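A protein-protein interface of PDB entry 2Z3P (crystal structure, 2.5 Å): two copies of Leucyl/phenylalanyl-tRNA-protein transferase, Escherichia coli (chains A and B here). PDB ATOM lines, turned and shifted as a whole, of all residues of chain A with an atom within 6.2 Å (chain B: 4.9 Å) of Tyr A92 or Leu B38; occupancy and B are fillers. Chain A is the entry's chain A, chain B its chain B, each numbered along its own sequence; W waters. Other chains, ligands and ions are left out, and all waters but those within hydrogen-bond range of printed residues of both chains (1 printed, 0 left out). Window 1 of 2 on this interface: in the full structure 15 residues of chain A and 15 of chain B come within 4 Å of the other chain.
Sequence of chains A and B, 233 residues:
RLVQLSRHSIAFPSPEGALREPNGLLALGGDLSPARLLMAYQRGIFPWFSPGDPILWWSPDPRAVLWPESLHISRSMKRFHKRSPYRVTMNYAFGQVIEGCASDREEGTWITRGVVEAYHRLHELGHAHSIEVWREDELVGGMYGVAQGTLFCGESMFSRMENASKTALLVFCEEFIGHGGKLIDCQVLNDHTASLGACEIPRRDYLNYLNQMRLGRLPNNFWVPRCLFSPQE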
ATOM      1  N   THR A  89       4.807 -31.029  -3.529  1.00  0.00           N
ATOM      2  CA  THR A  89       4.479 -30.159  -4.649  1.00  0.00           C
ATOM      3  C   THR A  89       5.023 -28.771  -4.385  1.00  0.00           C
ATOM      4  O   THR A  89       5.406 -28.454  -3.267  1.00  0.00           O
ATOM      5  CB  THR A  89       2.947 -30.031  -4.851  1.00  0.00           C
ATOM      6  OG1 THR A  89       2.358 -29.457  -3.675  1.00  0.00           O
ATOM      7  CG2 THR A  89       2.319 -31.392  -5.113  1.00  0.00           C
ATOM      8  N   MET A  90       5.059 -27.950  -5.427  1.00  0.00           N
ATOM      9  CA  MET A  90       5.528 -26.579  -5.306  1.00  0.00           C
ATOM     10  C   MET A  90       4.380 -25.649  -5.673  1.00  0.00           C
ATOM     11  O   MET A  90       3.710 -25.854  -6.686  1.00  0.00           O
ATOM     12  CB  MET A  90       6.713 -26.325  -6.237  1.00  0.00           C
ATOM     13  CG  MET A  90       7.206 -24.885  -6.223  1.00  0.00           C
ATOM     14  SD  MET A  90       8.608 -24.628  -7.347  1.00  0.00           S
ATOM     15  CE  MET A  90       9.998 -25.025  -6.240  1.00  0.00           C
ATOM     16  N   ASN A  91       4.156 -24.645  -4.834  1.00  0.00           N
ATOM     17  CA  ASN A  91       3.103 -23.657  -5.036  1.00  0.00           C
ATOM     18  C   ASN A  91       1.704 -24.162  -5.384  1.00  0.00           C
ATOM     19  O   ASN A  91       0.981 -23.520  -6.135  1.00  0.00           O
ATOM     20  CB  ASN A  91       3.542 -22.631  -6.079  1.00  0.00           C
ATOM     21  CG  ASN A  91       4.584 -21.685  -5.543  1.00  0.00           C
ATOM     22  OD1 ASN A  91       4.469 -21.205  -4.416  1.00  0.00           O
ATOM     23  ND2 ASN A  91       5.612 -21.412  -6.339  1.00  0.00           N
ATOM     24  N   TYR A  92       1.316 -25.304  -4.830  1.00  0.00           N
ATOM     25  CA  TYR A  92      -0.015 -25.843  -5.073  1.00  0.00           C
ATOM     26  C   TYR A  92      -0.979 -25.129  -4.139  1.00  0.00           C
ATOM     27  O   TYR A  92      -2.109 -24.852  -4.512  1.00  0.00           O
ATOM     28  CB  TYR A  92      -0.063 -27.337  -4.752  1.00  0.00           C
ATOM     29  CG  TYR A  92      -0.032 -28.259  -5.937  1.00  0.00           C
ATOM     30  CD1 TYR A  92       0.811 -28.013  -7.018  1.00  0.00           C
ATOM     31  CD2 TYR A  92      -0.802 -29.420  -5.953  1.00  0.00           C
ATOM     32  CE1 TYR A  92       0.892 -28.896  -8.078  1.00  0.00           C
ATOM     33  CE2 TYR A  92      -0.729 -30.312  -7.010  1.00  0.00           C
ATOM     34  CZ  TYR A  92       0.122 -30.043  -8.068  1.00  0.00           C
ATOM     35  OH  TYR A  92       0.218 -30.920  -9.119  1.00  0.00           O
ATOM     36  N   ALA A  93      -0.531 -24.835  -2.919  1.00  0.00           N
ATOM     37  CA  ALA A  93      -1.409 -24.203  -1.938  1.00  0.00           C
ATOM     38  C   ALA A  93      -0.708 -23.321  -0.912  1.00  0.00           C
ATOM     39  O   ALA A  93      -0.677 -23.650   0.274  1.00  0.00           O
ATOM     40  CB  ALA A  93      -2.221 -25.287  -1.211  1.00  0.00           C
ATOM     41  N   PHE A  94      -0.171 -22.195  -1.365  1.00  0.00           N
ATOM     42  CA  PHE A  94       0.530 -21.258  -0.498  1.00  0.00           C
ATOM     43  C   PHE A  94      -0.305 -20.868   0.722  1.00  0.00           C
ATOM     44  O   PHE A  94       0.186 -20.896   1.851  1.00  0.00           O
ATOM     45  CB  PHE A  94       0.892 -19.999  -1.293  1.00  0.00           C
ATOM     46  CG  PHE A  94       1.710 -19.017  -0.520  1.00  0.00           C
ATOM     47  CD1 PHE A  94       3.098 -19.119  -0.494  1.00  0.00           C
ATOM     48  CD2 PHE A  94       1.090 -18.009   0.217  1.00  0.00           C
ATOM     49  CE1 PHE A  94       3.865 -18.232   0.256  1.00  0.00           C
ATOM     50  CE2 PHE A  94       1.840 -17.116   0.973  1.00  0.00           C
ATOM     51  CZ  PHE A  94       3.238 -17.227   0.994  1.00  0.00           C
ATOM     52  N   SER A 130       5.761 -21.594  -1.917  1.00  0.00           N
ATOM     53  CA  SER A 130       5.553 -22.597  -0.886  1.00  0.00           C
ATOM     54  C   SER A 130       5.828 -24.016  -1.383  1.00  0.00           C
ATOM     55  O   SER A 130       5.748 -24.293  -2.579  1.00  0.00           O
ATOM     56  CB  SER A 130       4.117 -22.494  -0.345  1.00  0.00           C
ATOM     57  OG  SER A 130       3.167 -22.660  -1.375  1.00  0.00           O
ATOM     58  N   GLU A 132       4.583 -27.873  -0.543  1.00  0.00           N
ATOM     59  CA  GLU A 132       3.568 -28.644   0.167  1.00  0.00           C
ATOM     60  C   GLU A 132       3.925 -30.114   0.274  1.00  0.00           C
ATOM     61  O   GLU A 132       4.576 -30.678  -0.611  1.00  0.00           O
ATOM     62  CB  GLU A 132       2.206 -28.555  -0.544  1.00  0.00           C
ATOM     63  CG  GLU A 132       1.639 -27.157  -0.699  1.00  0.00           C
ATOM     64  CD  GLU A 132       2.257 -26.393  -1.851  1.00  0.00           C
ATOM     65  OE1 GLU A 132       2.343 -25.154  -1.746  1.00  0.00           O
ATOM     66  OE2 GLU A 132       2.643 -27.020  -2.862  1.00  0.00           O
ATOM     67  N   TRP A 134       1.997 -33.720   0.892  1.00  0.00           N
ATOM     68  CA  TRP A 134       0.706 -34.367   0.990  1.00  0.00           C
ATOM     69  C   TRP A 134       0.808 -35.819   1.387  1.00  0.00           C
ATOM     70  O   TRP A 134       1.731 -36.537   0.983  1.00  0.00           O
ATOM     71  CB  TRP A 134      -0.060 -34.298  -0.340  1.00  0.00           C
ATOM     72  CG  TRP A 134      -0.096 -32.950  -0.948  1.00  0.00           C
ATOM     73  CD1 TRP A 134       0.842 -32.396  -1.776  1.00  0.00           C
ATOM     74  CD2 TRP A 134      -1.108 -31.958  -0.760  1.00  0.00           C
ATOM     75  NE1 TRP A 134       0.472 -31.114  -2.118  1.00  0.00           N
ATOM     76  CE2 TRP A 134      -0.719 -30.818  -1.509  1.00  0.00           C
ATOM     77  CE3 TRP A 134      -2.308 -31.917  -0.031  1.00  0.00           C
ATOM     78  CZ2 TRP A 134      -1.489 -29.642  -1.547  1.00  0.00           C
ATOM     79  CZ3 TRP A 134      -3.077 -30.741  -0.066  1.00  0.00           C
ATOM     80  CH2 TRP A 134      -2.656 -29.621  -0.823  1.00  0.00           C
ATOM     81  N   PRO A 225       3.738 -23.720 -10.492  1.00  0.00           N
ATOM     82  CA  PRO A 225       3.193 -24.849  -9.728  1.00  0.00           C
ATOM     83  C   PRO A 225       3.451 -26.183 -10.399  1.00  0.00           C
ATOM     84  O   PRO A 225       3.259 -26.322 -11.599  1.00  0.00           O
ATOM     85  CB  PRO A 225       1.703 -24.516  -9.619  1.00  0.00           C
ATOM     86  CG  PRO A 225       1.461 -23.581 -10.779  1.00  0.00           C
ATOM     87  CD  PRO A 225       2.695 -22.727 -10.782  1.00  0.00           C
ATOM     88  N   ARG A 226       3.896 -27.159  -9.613  1.00  0.00           N
ATOM     89  CA  ARG A 226       4.198 -28.490 -10.131  1.00  0.00           C
ATOM     90  C   ARG A 226       4.465 -29.497  -9.012  1.00  0.00           C
ATOM     91  O   ARG A 226       4.611 -29.136  -7.839  1.00  0.00           O
ATOM     92  CB  ARG A 226       5.426 -28.422 -11.045  1.00  0.00           C
ATOM     93  CG  ARG A 226       6.693 -27.932 -10.346  1.00  0.00           C
ATOM     94  CD  ARG A 226       7.612 -27.209 -11.318  1.00  0.00           C
ATOM     95  NE  ARG A 226       8.731 -26.536 -10.654  1.00  0.00           N
ATOM     96  CZ  ARG A 226       9.883 -27.123 -10.350  1.00  0.00           C
ATOM     97  NH1 ARG A 226      10.078 -28.403 -10.655  1.00  0.00           N
ATOM     98  NH2 ARG A 226      10.845 -26.432  -9.750  1.00  0.00           N
ATOM     99  N   CYS A 227       4.533 -30.767  -9.392  1.00  0.00           N
ATOM    100  CA  CYS A 227       4.808 -31.845  -8.458  1.00  0.00           C
ATOM    101  C   CYS A 227       6.330 -32.009  -8.452  1.00  0.00           C
ATOM    102  O   CYS A 227       6.959 -31.978  -9.509  1.00  0.00           O
ATOM    103  CB  CYS A 227       4.128 -33.130  -8.947  1.00  0.00           C
ATOM    104  SG  CYS A 227       4.032 -34.486  -7.747  1.00  0.00           S
ATOM    105  N   PRO B  34      -8.617 -29.731  -3.382  1.00  0.00           N
ATOM    106  CA  PRO B  34      -7.672 -28.949  -4.181  1.00  0.00           C
ATOM    107  C   PRO B  34      -6.570 -29.788  -4.823  1.00  0.00           C
ATOM    108  O   PRO B  34      -6.259 -29.623  -6.007  1.00  0.00           O
ATOM    109  CB  PRO B  34      -7.117 -27.944  -3.173  1.00  0.00           C
ATOM    110  CG  PRO B  34      -8.250 -27.738  -2.255  1.00  0.00           C
ATOM    111  CD  PRO B  34      -8.800 -29.128  -2.052  1.00  0.00           C
ATOM    112  N   ALA B  35      -5.990 -30.691  -4.041  1.00  0.00           N
ATOM    113  CA  ALA B  35      -4.909 -31.533  -4.529  1.00  0.00           C
ATOM    114  C   ALA B  35      -5.342 -32.531  -5.599  1.00  0.00           C
ATOM    115  O   ALA B  35      -4.608 -32.762  -6.568  1.00  0.00           O
ATOM    116  CB  ALA B  35      -4.245 -32.269  -3.356  1.00  0.00           C
ATOM    117  N   ARG B  36      -6.525 -33.120  -5.441  1.00  0.00           N
ATOM    118  CA  ARG B  36      -6.987 -34.098  -6.424  1.00  0.00           C
ATOM    119  C   ARG B  36      -7.386 -33.443  -7.750  1.00  0.00           C
ATOM    120  O   ARG B  36      -7.248 -34.042  -8.819  1.00  0.00           O
ATOM    121  CB  ARG B  36      -8.157 -34.916  -5.875  1.00  0.00           C
ATOM    122  CG  ARG B  36      -8.556 -36.027  -6.812  1.00  0.00           C
ATOM    123  CD  ARG B  36      -9.784 -36.765  -6.344  1.00  0.00           C
ATOM    124  NE  ARG B  36      -9.456 -37.996  -5.633  1.00  0.00           N
ATOM    125  CZ  ARG B  36      -9.292 -38.078  -4.322  1.00  0.00           C
ATOM    126  NH1 ARG B  36      -9.425 -36.994  -3.571  1.00  0.00           N
ATOM    127  NH2 ARG B  36      -9.020 -39.245  -3.761  1.00  0.00           N
ATOM    128  N   LEU B  37      -7.881 -32.213  -7.686  1.00  0.00           N
ATOM    129  CA  LEU B  37      -8.270 -31.514  -8.904  1.00  0.00           C
ATOM    130  C   LEU B  37      -7.022 -31.120  -9.682  1.00  0.00           C
ATOM    131  O   LEU B  37      -6.956 -31.296 -10.897  1.00  0.00           O
ATOM    132  CB  LEU B  37      -9.094 -30.263  -8.576  1.00  0.00           C
ATOM    133  CG  LEU B  37     -10.551 -30.507  -8.198  1.00  0.00           C
ATOM    134  CD1 LEU B  37     -11.234 -29.164  -7.997  1.00  0.00           C
ATOM    135  CD2 LEU B  37     -11.256 -31.317  -9.286  1.00  0.00           C
ATOM    136  N   LEU B  38      -6.034 -30.583  -8.972  1.00  0.00           N
ATOM    137  CA  LEU B  38      -4.789 -30.182  -9.607  1.00  0.00           C
ATOM    138  C   LEU B  38      -4.133 -31.387 -10.243  1.00  0.00           C
ATOM    139  O   LEU B  38      -3.673 -31.317 -11.381  1.00  0.00           O
ATOM    140  CB  LEU B  38      -3.850 -29.543  -8.588  1.00  0.00           C
ATOM    141  CG  LEU B  38      -3.921 -28.017  -8.491  1.00  0.00           C
ATOM    142  CD1 LEU B  38      -5.327 -27.517  -8.749  1.00  0.00           C
ATOM    143  CD2 LEU B  38      -3.460 -27.605  -7.122  1.00  0.00           C
ATOM    144  N   MET B  39      -4.093 -32.499  -9.516  1.00  0.00           N
ATOM    145  CA  MET B  39      -3.507 -33.704 -10.072  1.00  0.00           C
ATOM    146  C   MET B  39      -4.233 -34.040 -11.370  1.00  0.00           C
ATOM    147  O   MET B  39      -3.606 -34.331 -12.392  1.00  0.00           O
ATOM    148  CB  MET B  39      -3.628 -34.854  -9.082  1.00  0.00           C
ATOM    149  CG  MET B  39      -2.579 -34.821  -7.975  1.00  0.00           C
ATOM    150  SD  MET B  39      -0.886 -35.079  -8.599  1.00  0.00           S
ATOM    151  CE  MET B  39      -0.127 -33.525  -8.192  1.00  0.00           C
ATOM    152  N   ALA B  40      -5.559 -33.971 -11.331  1.00  0.00           N
ATOM    153  CA  ALA B  40      -6.378 -34.274 -12.498  1.00  0.00           C
ATOM    154  C   ALA B  40      -6.042 -33.380 -13.686  1.00  0.00           C
ATOM    155  O   ALA B  40      -5.674 -33.882 -14.752  1.00  0.00           O
ATOM    156  CB  ALA B  40      -7.853 -34.146 -12.150  1.00  0.00           C
ATOM    157  N   TYR B  41      -6.174 -32.064 -13.501  1.00  0.00           N
ATOM    158  CA  TYR B  41      -5.896 -31.104 -14.571  1.00  0.00           C
ATOM    159  C   TYR B  41      -4.492 -31.270 -15.117  1.00  0.00           C
ATOM    160  O   TYR B  41      -4.245 -31.076 -16.310  1.00  0.00           O
ATOM    161  CB  TYR B  41      -6.112 -29.669 -14.078  1.00  0.00           C
ATOM    162  CG  TYR B  41      -7.579 -29.297 -14.038  1.00  0.00           C
ATOM    163  CD1 TYR B  41      -8.269 -28.979 -15.212  1.00  0.00           C
ATOM    164  CD2 TYR B  41      -8.300 -29.357 -12.844  1.00  0.00           C
ATOM    165  CE1 TYR B  41      -9.640 -28.738 -15.195  1.00  0.00           C
ATOM    166  CE2 TYR B  41      -9.667 -29.121 -12.816  1.00  0.00           C
ATOM    167  CZ  TYR B  41     -10.333 -28.815 -13.992  1.00  0.00           C
ATOM    168  OH  TYR B  41     -11.695 -28.611 -13.959  1.00  0.00           O
ATOM    169  N   GLN B  42      -3.583 -31.654 -14.233  1.00  0.00           N
ATOM    170  CA  GLN B  42      -2.192 -31.879 -14.591  1.00  0.00           C
ATOM    171  C   GLN B  42      -2.058 -33.068 -15.535  1.00  0.00           C
ATOM    172  O   GLN B  42      -1.081 -33.164 -16.272  1.00  0.00           O
ATOM    173  CB  GLN B  42      -1.386 -32.143 -13.326  1.00  0.00           C
ATOM    174  CG  GLN B  42       0.069 -32.483 -13.544  1.00  0.00           C
ATOM    175  CD  GLN B  42       0.791 -32.683 -12.228  1.00  0.00           C
ATOM    176  OE1 GLN B  42       2.015 -32.833 -12.180  1.00  0.00           O
ATOM    177  NE2 GLN B  42       0.028 -32.687 -11.143  1.00  0.00           N
ATOM    178  N   LEU B 122      -9.859 -23.466  -5.561  1.00  0.00           N
ATOM    179  CA  LEU B 122      -8.781 -23.372  -6.529  1.00  0.00           C
ATOM    180  C   LEU B 122      -8.541 -21.911  -6.875  1.00  0.00           C
ATOM    181  O   LEU B 122      -7.405 -21.492  -7.103  1.00  0.00           O
ATOM    182  CB  LEU B 122      -9.125 -24.144  -7.787  1.00  0.00           C
ATOM    183  CG  LEU B 122      -9.129 -25.664  -7.635  1.00  0.00           C
ATOM    184  CD1 LEU B 122      -9.360 -26.324  -9.010  1.00  0.00           C
ATOM    185  CD2 LEU B 122      -7.798 -26.111  -7.030  1.00  0.00           C
ATOM    186  N   LEU B 125      -6.704 -20.519  -4.036  1.00  0.00           N
ATOM    187  CA  LEU B 125      -5.332 -20.999  -4.038  1.00  0.00           C
ATOM    188  C   LEU B 125      -4.576 -20.469  -5.258  1.00  0.00           C
ATOM    189  O   LEU B 125      -3.373 -20.696  -5.398  1.00  0.00           O
ATOM    190  CB  LEU B 125      -5.303 -22.531  -3.998  1.00  0.00           C
ATOM    191  CG  LEU B 125      -5.897 -23.069  -2.680  1.00  0.00           C
ATOM    192  CD1 LEU B 125      -5.968 -24.604  -2.689  1.00  0.00           C
ATOM    193  CD2 LEU B 125      -5.039 -22.570  -1.509  1.00  0.00           C
ATOM    194  N   HIS B 127      -5.344 -21.002  -8.775  1.00  0.00           N
ATOM    195  CA  HIS B 127      -5.282 -21.810  -9.992  1.00  0.00           C
ATOM    196  C   HIS B 127      -6.513 -21.667 -10.892  1.00  0.00           C
ATOM    197  O   HIS B 127      -6.439 -21.948 -12.089  1.00  0.00           O
ATOM    198  CB  HIS B 127      -5.087 -23.289  -9.640  1.00  0.00           C
ATOM    199  CG  HIS B 127      -3.832 -23.555  -8.880  1.00  0.00           C
ATOM    200  ND1 HIS B 127      -3.809 -23.715  -7.511  1.00  0.00           N
ATOM    201  CD2 HIS B 127      -2.544 -23.621  -9.289  1.00  0.00           C
ATOM    202  CE1 HIS B 127      -2.561 -23.866  -7.111  1.00  0.00           C
ATOM    203  NE2 HIS B 127      -1.774 -23.811  -8.169  1.00  0.00           N
ATOM    204  N   GLN B 148      -3.174 -23.786 -16.461  1.00  0.00           N
ATOM    205  CA  GLN B 148      -2.241 -24.891 -16.546  1.00  0.00           C
ATOM    206  C   GLN B 148      -1.063 -24.351 -17.351  1.00  0.00           C
ATOM    207  O   GLN B 148      -0.848 -24.742 -18.495  1.00  0.00           O
ATOM    208  CB  GLN B 148      -2.922 -26.032 -17.303  1.00  0.00           C
ATOM    209  CG  GLN B 148      -2.615 -27.429 -16.832  1.00  0.00           C
ATOM    210  CD  GLN B 148      -2.807 -27.594 -15.350  1.00  0.00           C
ATOM    211  OE1 GLN B 148      -3.765 -27.073 -14.775  1.00  0.00           O
ATOM    212  NE2 GLN B 148      -1.895 -28.327 -14.716  1.00  0.00           N
HETATM  213  O   HOH W   1      -0.821 -21.574  -4.088  1.00  0.00           O
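NE2 of His B127 sits at hydrogen-bond distance from O of Asn A91, 3.4 Å away. The side-chain hydroxyl of Tyr A92 sits at hydrogen-bond distance from the side-chain amide nitrogen of Gln B42, 2.7 Å away.
OG1 of Thr A89 is in hydrogen-bond range of NE1 of Trp A134. N of Asn A91 sits at hydrogen-bond distance from OE2 of Glu A132, at 3.4 Å. N of Tyr A92 lies within hydrogen-bond range of OE2 of Glu A132, 2.9 Å away. The backbone NH (N) of Ala A93 sits at hydrogen-bond distance from the side-chain carboxylate (OE1) of Glu A132, 3.1 Å away. The side-chain amide nitrogen (NE2) of Gln B42 sits close to the side-chain sulfur (SD) of Met B39 (3.6 Å). The backbone NH of His B127 lies within hydrogen-bond range of the backbone carbonyl oxygen of Leu B122.
Leu B38 touches Tyr A92. Tyr A92 touches Met B39 (OH to CE, 2.8 Å). Tyr A92 touches Leu B125. Tyr A92 touches His B127. Ala A93 touches Leu B125 (CB to CD2, 3.9 Å). Ala B35 touches Trp A134 (CB to CZ3, 3.8 Å). NE2 of His B127 touches CB of Pro A225, 3.8 Å away. Cys A227 touches Gln B42 (CB to OE1, 3.9 Å).
Printed residues of chain B within 4 Å of Tyr A92: Leu B38, Met B39, Gln B42, Leu B125 and His B127. Of the printed residues of chain B, Trp A134 touches Ala B35. Of the printed residues of chain B, Cys A227 touches Gln B42. Leu B38 touches just one residue of chain A: Tyr A92 (3.4 Å). Of the printed residues of chain A, Met B39 touches Tyr A92. Tyr B41 touches none of the printed residues of chain A. Printed residues of chain A within 4 Å of Leu B125: Tyr A92 and Ala A93. Printed residues of chain A within 4 Å of His B127: Asn A91 (3.4 Å), Tyr A92 (2.8 Å) and Pro A225 (3.8 Å). The nearest printed residue of chain B that does not touch Tyr A92 is Ala B35 (4.6 Å). The nearest printed residue of chain A that does not touch Met B39 is Cys A227 (4.3 Å).
Hydrophobic or aromatic side chains of chain B within 4 Å of the printed part of chain A: Ala B35, Leu B38, Met B39, Leu B125 and His B127. Along chain B the printed residues that touch a printed residue of chain A span positions 35 to 127. Of the 12 printed residues of chain A, 6 touch a printed residue of chain B. Printed residues of chain A that touch a printed residue of chain B: Asn A91, Tyr A92, Ala A93, Trp A134, Pro A225 and Cys A227.
No position is printed for both chains. Of the 10 pairs that touch across the chains among the printed residues, none has its exchanged pair printed and touching as well.
Water W1 lies within hydrogen-bond range of N of Phe A94 (2.9 Å), O of Leu B125 (3.0 Å), O of Asn A91 (3.4 Å) and N of Ala A93 (3.5 Å).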
